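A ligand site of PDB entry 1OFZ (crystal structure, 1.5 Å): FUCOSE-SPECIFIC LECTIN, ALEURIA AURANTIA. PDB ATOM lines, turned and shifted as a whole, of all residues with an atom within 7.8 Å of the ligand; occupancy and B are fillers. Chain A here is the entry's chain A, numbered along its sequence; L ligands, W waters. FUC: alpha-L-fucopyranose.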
ATOM      1  N   ILE A 173     -26.641  -4.374  -5.240  1.00  0.00           N
ATOM      2  CA  ILE A 173     -27.630  -3.376  -4.809  1.00  0.00           C
ATOM      3  C   ILE A 173     -27.834  -2.281  -5.836  1.00  0.00           C
ATOM      4  O   ILE A 173     -28.783  -1.494  -5.721  1.00  0.00           O
ATOM      5  CB  ILE A 173     -27.243  -2.772  -3.418  1.00  0.00           C
ATOM      6  CG1 ILE A 173     -25.969  -1.920  -3.484  1.00  0.00           C
ATOM      7  CG2 ILE A 173     -27.082  -3.861  -2.386  1.00  0.00           C
ATOM      8  CD1 ILE A 173     -25.671  -1.141  -2.189  1.00  0.00           C
ATOM      9  N   ARG A 177     -22.513  -2.398  -7.995  1.00  0.00           N
ATOM     10  CA  ARG A 177     -22.427  -2.012  -6.592  1.00  0.00           C
ATOM     11  C   ARG A 177     -22.818  -3.233  -5.768  1.00  0.00           C
ATOM     12  O   ARG A 177     -23.952  -3.689  -5.815  1.00  0.00           O
ATOM     13  CB  ARG A 177     -23.408  -0.858  -6.327  1.00  0.00           C
ATOM     14  CG  ARG A 177     -23.219  -0.173  -5.024  1.00  0.00           C
ATOM     15  CD  ARG A 177     -24.054   1.144  -4.957  1.00  0.00           C
ATOM     16  NE  ARG A 177     -23.857   1.843  -3.703  1.00  0.00           N
ATOM     17  CZ  ARG A 177     -24.794   2.483  -3.023  1.00  0.00           C
ATOM     18  NH1 ARG A 177     -26.048   2.533  -3.475  1.00  0.00           N
ATOM     19  NH2 ARG A 177     -24.450   3.087  -1.910  1.00  0.00           N
ATOM     20  N   LEU A 178     -21.843  -3.779  -5.047  1.00  0.00           N
ATOM     21  CA  LEU A 178     -21.943  -5.115  -4.471  1.00  0.00           C
ATOM     22  C   LEU A 178     -21.890  -5.066  -2.973  1.00  0.00           C
ATOM     23  O   LEU A 178     -21.123  -4.315  -2.404  1.00  0.00           O
ATOM     24  CB  LEU A 178     -20.827  -6.008  -4.995  1.00  0.00           C
ATOM     25  CG  LEU A 178     -20.545  -5.943  -6.477  1.00  0.00           C
ATOM     26  CD1 LEU A 178     -19.387  -6.906  -6.864  1.00  0.00           C
ATOM     27  CD2 LEU A 178     -21.779  -6.220  -7.311  1.00  0.00           C
ATOM     28  N   ARG A 179     -22.639  -5.939  -2.306  1.00  0.00           N
ATOM     29  CA  ARG A 179     -22.584  -6.133  -0.875  1.00  0.00           C
ATOM     30  C   ARG A 179     -22.513  -7.591  -0.547  1.00  0.00           C
ATOM     31  O   ARG A 179     -23.322  -8.381  -1.031  1.00  0.00           O
ATOM     32  CB  ARG A 179     -23.776  -5.473  -0.178  1.00  0.00           C
ATOM     33  CG  ARG A 179     -23.874  -3.979  -0.334  1.00  0.00           C
ATOM     34  CD  ARG A 179     -22.717  -3.250   0.351  1.00  0.00           C
ATOM     35  NE  ARG A 179     -22.809  -1.792   0.258  1.00  0.00           N
ATOM     36  CZ  ARG A 179     -22.368  -1.060  -0.737  1.00  0.00           C
ATOM     37  NH1 ARG A 179     -21.800  -1.587  -1.798  1.00  0.00           N
ATOM     38  NH2 ARG A 179     -22.476   0.285  -0.686  1.00  0.00           N
ATOM     39  N   ILE A 180     -21.522  -7.960   0.240  1.00  0.00           N
ATOM     40  CA  ILE A 180     -21.252  -9.323   0.645  1.00  0.00           C
ATOM     41  C   ILE A 180     -21.350  -9.411   2.150  1.00  0.00           C
ATOM     42  O   ILE A 180     -20.703  -8.645   2.877  1.00  0.00           O
ATOM     43  CB  ILE A 180     -19.830  -9.781   0.186  1.00  0.00           C
ATOM     44  CG1 ILE A 180     -19.549  -9.481  -1.269  1.00  0.00           C
ATOM     45  CG2 ILE A 180     -19.607 -11.229   0.501  1.00  0.00           C
ATOM     46  CD1 ILE A 180     -20.514 -10.093  -2.240  1.00  0.00           C
ATOM     47  N   TYR A 181     -22.103 -10.401   2.634  1.00  0.00           N
ATOM     48  CA  TYR A 181     -22.324 -10.611   4.040  1.00  0.00           C
ATOM     49  C   TYR A 181     -21.785 -11.964   4.440  1.00  0.00           C
ATOM     50  O   TYR A 181     -21.944 -12.932   3.717  1.00  0.00           O
ATOM     51  CB  TYR A 181     -23.840 -10.483   4.388  1.00  0.00           C
ATOM     52  CG  TYR A 181     -24.350  -9.133   3.983  1.00  0.00           C
ATOM     53  CD1 TYR A 181     -24.247  -8.067   4.836  1.00  0.00           C
ATOM     54  CD2 TYR A 181     -24.860  -8.911   2.701  1.00  0.00           C
ATOM     55  CE1 TYR A 181     -24.602  -6.817   4.434  1.00  0.00           C
ATOM     56  CE2 TYR A 181     -25.226  -7.651   2.290  1.00  0.00           C
ATOM     57  CZ  TYR A 181     -25.074  -6.587   3.168  1.00  0.00           C
ATOM     58  OH  TYR A 181     -25.442  -5.308   2.767  1.00  0.00           O
ATOM     59  N   GLU A 191     -19.974  -7.015   6.711  1.00  0.00           N
ATOM     60  CA  GLU A 191     -20.340  -6.612   5.399  1.00  0.00           C
ATOM     61  C   GLU A 191     -19.110  -6.087   4.668  1.00  0.00           C
ATOM     62  O   GLU A 191     -18.330  -5.291   5.244  1.00  0.00           O
ATOM     63  CB  GLU A 191     -21.384  -5.497   5.501  1.00  0.00           C
ATOM     64  CG  GLU A 191     -21.813  -4.847   4.206  1.00  0.00           C
ATOM     65  CD  GLU A 191     -22.674  -3.627   4.424  1.00  0.00           C
ATOM     66  OE1 GLU A 191     -22.268  -2.753   5.226  1.00  0.00           O
ATOM     67  OE2 GLU A 191     -23.778  -3.557   3.842  1.00  0.00           O
ATOM     68  N   HIS A 192     -18.910  -6.529   3.441  1.00  0.00           N
ATOM     69  CA  HIS A 192     -17.898  -5.991   2.538  1.00  0.00           C
ATOM     70  C   HIS A 192     -18.573  -5.399   1.334  1.00  0.00           C
ATOM     71  O   HIS A 192     -19.562  -5.927   0.821  1.00  0.00           O
ATOM     72  CB  HIS A 192     -16.937  -7.059   2.104  1.00  0.00           C
ATOM     73  CG  HIS A 192     -15.533  -6.683   2.356  1.00  0.00           C
ATOM     74  ND1 HIS A 192     -15.000  -6.708   3.610  1.00  0.00           N
ATOM     75  CD2 HIS A 192     -14.576  -6.206   1.533  1.00  0.00           C
ATOM     76  CE1 HIS A 192     -13.746  -6.301   3.550  1.00  0.00           C
ATOM     77  NE2 HIS A 192     -13.474  -5.970   2.306  1.00  0.00           N
ATOM     78  N   CYS A 193     -18.041  -4.272   0.865  1.00  0.00           N
ATOM     79  CA  CYS A 193     -18.696  -3.409  -0.092  1.00  0.00           C
ATOM     80  C   CYS A 193     -17.804  -3.060  -1.266  1.00  0.00           C
ATOM     81  O   CYS A 193     -16.603  -2.812  -1.077  1.00  0.00           O
ATOM     82  CB  CYS A 193     -19.065  -2.095   0.560  1.00  0.00           C
ATOM     83  SG  CYS A 193     -19.928  -2.197   2.139  1.00  0.00           S
ATOM     84  N   ASP A 195     -18.264  -0.228  -4.398  1.00  0.00           N
ATOM     85  CA  ASP A 195     -19.077   0.783  -5.085  1.00  0.00           C
ATOM     86  C   ASP A 195     -18.528   1.193  -6.448  1.00  0.00           C
ATOM     87  O   ASP A 195     -19.291   1.468  -7.365  1.00  0.00           O
ATOM     88  CB  ASP A 195     -19.160   2.073  -4.239  1.00  0.00           C
ATOM     89  CG  ASP A 195     -20.032   1.935  -3.012  1.00  0.00           C
ATOM     90  OD1 ASP A 195     -21.033   1.163  -3.015  1.00  0.00           O
ATOM     91  OD2 ASP A 195     -19.798   2.618  -1.988  1.00  0.00           O
ATOM     92  N   TYR A 200     -14.274  -2.327   0.522  1.00  0.00           N
ATOM     93  CA  TYR A 200     -14.095  -1.748   1.842  1.00  0.00           C
ATOM     94  C   TYR A 200     -15.079  -2.346   2.811  1.00  0.00           C
ATOM     95  O   TYR A 200     -16.117  -2.929   2.432  1.00  0.00           O
ATOM     96  CB  TYR A 200     -14.269  -0.236   1.761  1.00  0.00           C
ATOM     97  CG  TYR A 200     -15.647   0.256   1.407  1.00  0.00           C
ATOM     98  CD1 TYR A 200     -16.600   0.504   2.394  1.00  0.00           C
ATOM     99  CD2 TYR A 200     -16.025   0.487   0.081  1.00  0.00           C
ATOM    100  CE1 TYR A 200     -17.857   0.961   2.075  1.00  0.00           C
ATOM    101  CE2 TYR A 200     -17.285   0.933  -0.246  1.00  0.00           C
ATOM    102  CZ  TYR A 200     -18.198   1.200   0.764  1.00  0.00           C
ATOM    103  OH  TYR A 200     -19.438   1.658   0.414  1.00  0.00           O
ATOM    104  N   VAL A 201     -14.770  -2.197   4.077  1.00  0.00           N
ATOM    105  CA  VAL A 201     -15.596  -2.737   5.138  1.00  0.00           C
ATOM    106  C   VAL A 201     -16.839  -1.863   5.350  1.00  0.00           C
ATOM    107  O   VAL A 201     -16.753  -0.654   5.610  1.00  0.00           O
ATOM    108  CB  VAL A 201     -14.796  -2.792   6.446  1.00  0.00           C
ATOM    109  CG1 VAL A 201     -15.684  -3.240   7.584  1.00  0.00           C
ATOM    110  CG2 VAL A 201     -13.626  -3.668   6.298  1.00  0.00           C
ATOM    111  N   GLY A 202     -18.016  -2.465   5.236  1.00  0.00           N
ATOM    112  CA  GLY A 202     -19.247  -1.739   5.419  1.00  0.00           C
ATOM    113  C   GLY A 202     -19.583  -1.463   6.869  1.00  0.00           C
ATOM    114  O   GLY A 202     -18.976  -2.047   7.793  1.00  0.00           O
ATOM    115  N   GLY A 203     -20.547  -0.573   7.081  1.00  0.00           N
ATOM    116  CA  GLY A 203     -20.983  -0.205   8.393  1.00  0.00           C
ATOM    117  C   GLY A 203     -21.782  -1.247   9.158  1.00  0.00           C
ATOM    118  O   GLY A 203     -21.968  -1.159  10.386  1.00  0.00           O
ATOM    119  N   PHE A 204     -22.317  -2.214   8.420  1.00  0.00           N
ATOM    120  CA  PHE A 204     -23.220  -3.175   9.038  1.00  0.00           C
ATOM    121  C   PHE A 204     -22.520  -4.229   9.851  1.00  0.00           C
ATOM    122  O   PHE A 204     -21.539  -4.780   9.395  1.00  0.00           O
ATOM    123  CB  PHE A 204     -24.065  -3.909   7.975  1.00  0.00           C
ATOM    124  CG  PHE A 204     -24.932  -4.983   8.557  1.00  0.00           C
ATOM    125  CD1 PHE A 204     -26.026  -4.645   9.345  1.00  0.00           C
ATOM    126  CD2 PHE A 204     -24.602  -6.329   8.420  1.00  0.00           C
ATOM    127  CE1 PHE A 204     -26.780  -5.614   9.926  1.00  0.00           C
ATOM    128  CE2 PHE A 204     -25.364  -7.289   9.029  1.00  0.00           C
ATOM    129  CZ  PHE A 204     -26.450  -6.942   9.752  1.00  0.00           C
ATOM    130  N   SER A 205     -23.007  -4.474  11.055  1.00  0.00           N
ATOM    131  CA  SER A 205     -22.615  -5.667  11.805  1.00  0.00           C
ATOM    132  C   SER A 205     -23.706  -6.047  12.786  1.00  0.00           C
ATOM    133  O   SER A 205     -24.475  -5.203  13.240  1.00  0.00           O
ATOM    134  CB  SER A 205     -21.256  -5.484  12.517  1.00  0.00           C
ATOM    135  OG  SER A 205     -21.394  -4.588  13.610  1.00  0.00           O
ATOM    136  N   THR A 222     -33.521   2.911  -3.563  1.00  0.00           N
ATOM    137  CA  THR A 222     -33.120   3.526  -2.294  1.00  0.00           C
ATOM    138  C   THR A 222     -31.631   3.345  -1.933  1.00  0.00           C
ATOM    139  O   THR A 222     -30.996   4.329  -1.520  1.00  0.00           O
ATOM    140  CB  THR A 222     -34.087   3.077  -1.191  1.00  0.00           C
ATOM    141  OG1 THR A 222     -35.419   3.606  -1.437  1.00  0.00           O
ATOM    142  CG2 THR A 222     -33.642   3.604   0.204  1.00  0.00           C
ATOM    143  N   PRO A 223     -31.039   2.146  -2.040  1.00  0.00           N
ATOM    144  CA  PRO A 223     -31.719   0.877  -2.293  1.00  0.00           C
ATOM    145  C   PRO A 223     -32.116   0.211  -0.989  1.00  0.00           C
ATOM    146  O   PRO A 223     -31.812   0.694   0.098  1.00  0.00           O
ATOM    147  CB  PRO A 223     -30.621   0.052  -2.973  1.00  0.00           C
ATOM    148  CG  PRO A 223     -29.417   0.498  -2.247  1.00  0.00           C
ATOM    149  CD  PRO A 223     -29.595   1.937  -1.841  1.00  0.00           C
ATOM    150  N   ASN A 224     -32.781  -0.939  -1.102  1.00  0.00           N
ATOM    151  CA  ASN A 224     -33.246  -1.710   0.032  1.00  0.00           C
ATOM    152  C   ASN A 224     -32.459  -3.005   0.075  1.00  0.00           C
ATOM    153  O   ASN A 224     -32.246  -3.620  -0.943  1.00  0.00           O
ATOM    154  CB  ASN A 224     -34.737  -2.022  -0.094  1.00  0.00           C
ATOM    155  CG  ASN A 224     -35.529  -0.778  -0.327  1.00  0.00           C
ATOM    156  OD1 ASN A 224     -35.879  -0.070   0.615  1.00  0.00           O
ATOM    157  ND2 ASN A 224     -35.824  -0.504  -1.616  1.00  0.00           N
ATOM    158  N   ILE A 225     -31.949  -3.338   1.251  1.00  0.00           N
ATOM    159  CA  ILE A 225     -31.177  -4.559   1.457  1.00  0.00           C
ATOM    160  C   ILE A 225     -31.833  -5.304   2.581  1.00  0.00           C
ATOM    161  O   ILE A 225     -32.286  -4.702   3.598  1.00  0.00           O
ATOM    162  CB  ILE A 225     -29.695  -4.275   1.842  1.00  0.00           C
ATOM    163  CG1 ILE A 225     -29.094  -3.189   0.954  1.00  0.00           C
ATOM    164  CG2 ILE A 225     -28.873  -5.578   1.720  1.00  0.00           C
ATOM    165  CD1 ILE A 225     -27.716  -2.760   1.341  1.00  0.00           C
ATOM    166  N   TYR A 241     -32.081  -2.624   5.549  1.00  0.00           N
ATOM    167  CA  TYR A 241     -31.506  -1.338   5.203  1.00  0.00           C
ATOM    168  C   TYR A 241     -32.446  -0.645   4.233  1.00  0.00           C
ATOM    169  O   TYR A 241     -32.831  -1.205   3.221  1.00  0.00           O
ATOM    170  CB  TYR A 241     -30.162  -1.532   4.488  1.00  0.00           C
ATOM    171  CG  TYR A 241     -29.474  -0.250   4.097  1.00  0.00           C
ATOM    172  CD1 TYR A 241     -28.607   0.406   4.985  1.00  0.00           C
ATOM    173  CD2 TYR A 241     -29.646   0.277   2.843  1.00  0.00           C
ATOM    174  CE1 TYR A 241     -27.925   1.570   4.615  1.00  0.00           C
ATOM    175  CE2 TYR A 241     -28.990   1.472   2.450  1.00  0.00           C
ATOM    176  CZ  TYR A 241     -28.116   2.079   3.344  1.00  0.00           C
ATOM    177  OH  TYR A 241     -27.481   3.256   2.958  1.00  0.00           O
ATOM    178  N   GLY A 243     -31.594   2.965   3.807  1.00  0.00           N
ATOM    179  CA  GLY A 243     -30.856   4.196   3.943  1.00  0.00           C
ATOM    180  C   GLY A 243     -30.084   4.216   5.241  1.00  0.00           C
ATOM    181  O   GLY A 243     -29.024   4.853   5.382  1.00  0.00           O
ATOM    182  N   SER A 244     -30.639   3.485   6.195  1.00  0.00           N
ATOM    183  CA  SER A 244     -29.980   3.158   7.452  1.00  0.00           C
ATOM    184  C   SER A 244     -30.320   1.719   7.814  1.00  0.00           C
ATOM    185  O   SER A 244     -31.310   1.162   7.306  1.00  0.00           O
ATOM    186  CB  SER A 244     -30.406   4.133   8.552  1.00  0.00           C
ATOM    187  OG  SER A 244     -31.773   3.957   8.884  1.00  0.00           O
ATOM    188  N   TRP A 245     -29.554   1.118   8.710  1.00  0.00           N
ATOM    189  CA  TRP A 245     -29.849  -0.229   9.203  1.00  0.00           C
ATOM    190  C   TRP A 245     -30.768  -0.185  10.386  1.00  0.00           C
ATOM    191  O   TRP A 245     -30.651   0.685  11.266  1.00  0.00           O
ATOM    192  CB  TRP A 245     -28.594  -1.016   9.557  1.00  0.00           C
ATOM    193  CG  TRP A 245     -27.786  -1.388   8.380  1.00  0.00           C
ATOM    194  CD1 TRP A 245     -26.690  -0.733   7.912  1.00  0.00           C
ATOM    195  CD2 TRP A 245     -28.010  -2.480   7.478  1.00  0.00           C
ATOM    196  NE1 TRP A 245     -26.214  -1.344   6.774  1.00  0.00           N
ATOM    197  CE2 TRP A 245     -27.010  -2.417   6.480  1.00  0.00           C
ATOM    198  CE3 TRP A 245     -28.950  -3.518   7.409  1.00  0.00           C
ATOM    199  CZ2 TRP A 245     -26.920  -3.358   5.443  1.00  0.00           C
ATOM    200  CZ3 TRP A 245     -28.830  -4.462   6.366  1.00  0.00           C
ATOM    201  CH2 TRP A 245     -27.851  -4.355   5.414  1.00  0.00           C
HETATM  202  C1  FUC L   1     -22.427   1.643   2.756  1.00  0.00           C
HETATM  203  C2  FUC L   1     -22.349   0.598   3.878  1.00  0.00           C
HETATM  204  C3  FUC L   1     -23.739   0.333   4.438  1.00  0.00           C
HETATM  205  C4  FUC L   1     -24.699  -0.032   3.296  1.00  0.00           C
HETATM  206  C5  FUC L   1     -24.711   1.080   2.246  1.00  0.00           C
HETATM  207  C6  FUC L   1     -25.629   0.792   1.055  1.00  0.00           C
HETATM  208  O1  FUC L   1     -22.764   2.892   3.339  1.00  0.00           O
HETATM  209  O2  FUC L   1     -21.451   1.020   4.906  1.00  0.00           O
HETATM  210  O3  FUC L   1     -23.746  -0.616   5.500  1.00  0.00           O
HETATM  211  O4  FUC L   1     -24.242  -1.221   2.650  1.00  0.00           O
HETATM  212  O5  FUC L   1     -23.397   1.285   1.761  1.00  0.00           O
HETATM  213  O   HOH W   1     -25.440   4.078   4.836  1.00  0.00           O
HETATM  214  O   HOH W   2     -23.819   1.010   7.770  1.00  0.00           O
HETATM  215  O   HOH W   3     -22.382   3.391   6.370  1.00  0.00           O
HETATM  216  O   HOH W   4     -19.845   3.155   4.377  1.00  0.00           O
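O3 of the ligand sits at hydrogen-bond distance from OE1 of Glu 191, at 2.6 Å.
NH2 of Arg 179 is in hydrogen-bond range of O5 of the ligand.
The backbone NH (N) of Gly 203 is in hydrogen-bond range of an oxygen (O2) of the ligand (2.8 Å).
The indole nitrogen of Trp 245 is in hydrogen-bond range of an oxygen (O3) of the ligand (2.9 Å).
The side-chain carboxylate of Glu 191 lies within hydrogen-bond range of the backbone NH of Gly 203 (3.3 Å).
The backbone NH (N) of Gly 202 is in hydrogen-bond range of the backbone carbonyl oxygen (O) of Glu 191 (2.8 Å).
N of Phe 204 sits at hydrogen-bond distance from OE1 of Glu 191.
The guanidinium group (NH2) of Arg 179 lies within salt-bridge range of the side-chain carboxylate (OD1) of Asp 195 (2.9 Å).
The backbone carbonyl oxygen (O) of Ile 225 sits at hydrogen-bond distance from the backbone NH (N) of Tyr 241 (2.9 Å).
O of Gly 243 lies within hydrogen-bond range of OH of Tyr 241 (3.3 Å).
The backbone carbonyl oxygen (O) of Tyr 200 sits at hydrogen-bond distance from the backbone NH (N) of Cys 193, 2.8 Å away.
OH of Tyr 200 is in hydrogen-bond range of OD2 of Asp 195 (2.6 Å).
Merely in contact with the ligand: Ile 173, Arg 177, Tyr 200, Gly 202, Phe 204 and Tyr 241.
Hydrophobic or aromatic side chains that line the ligand: Ile 173, Tyr 241 and Trp 245.
Ten residues have an atom within 4 Å of the ligand: Ile 173, Arg 177, Arg 179, Glu 191, Tyr 200, Gly 202, Gly 203, Phe 204, Tyr 241 and Trp 245.
Along chain A the residues within 4 Å of the ligand span positions 173 to 245.
The nearest printed residue that does not touch the ligand is Ile 225 (4.02 Å).
Water W1 bridges OH of Tyr 241 (2.9 Å) and O1 of the ligand (3.3 Å).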
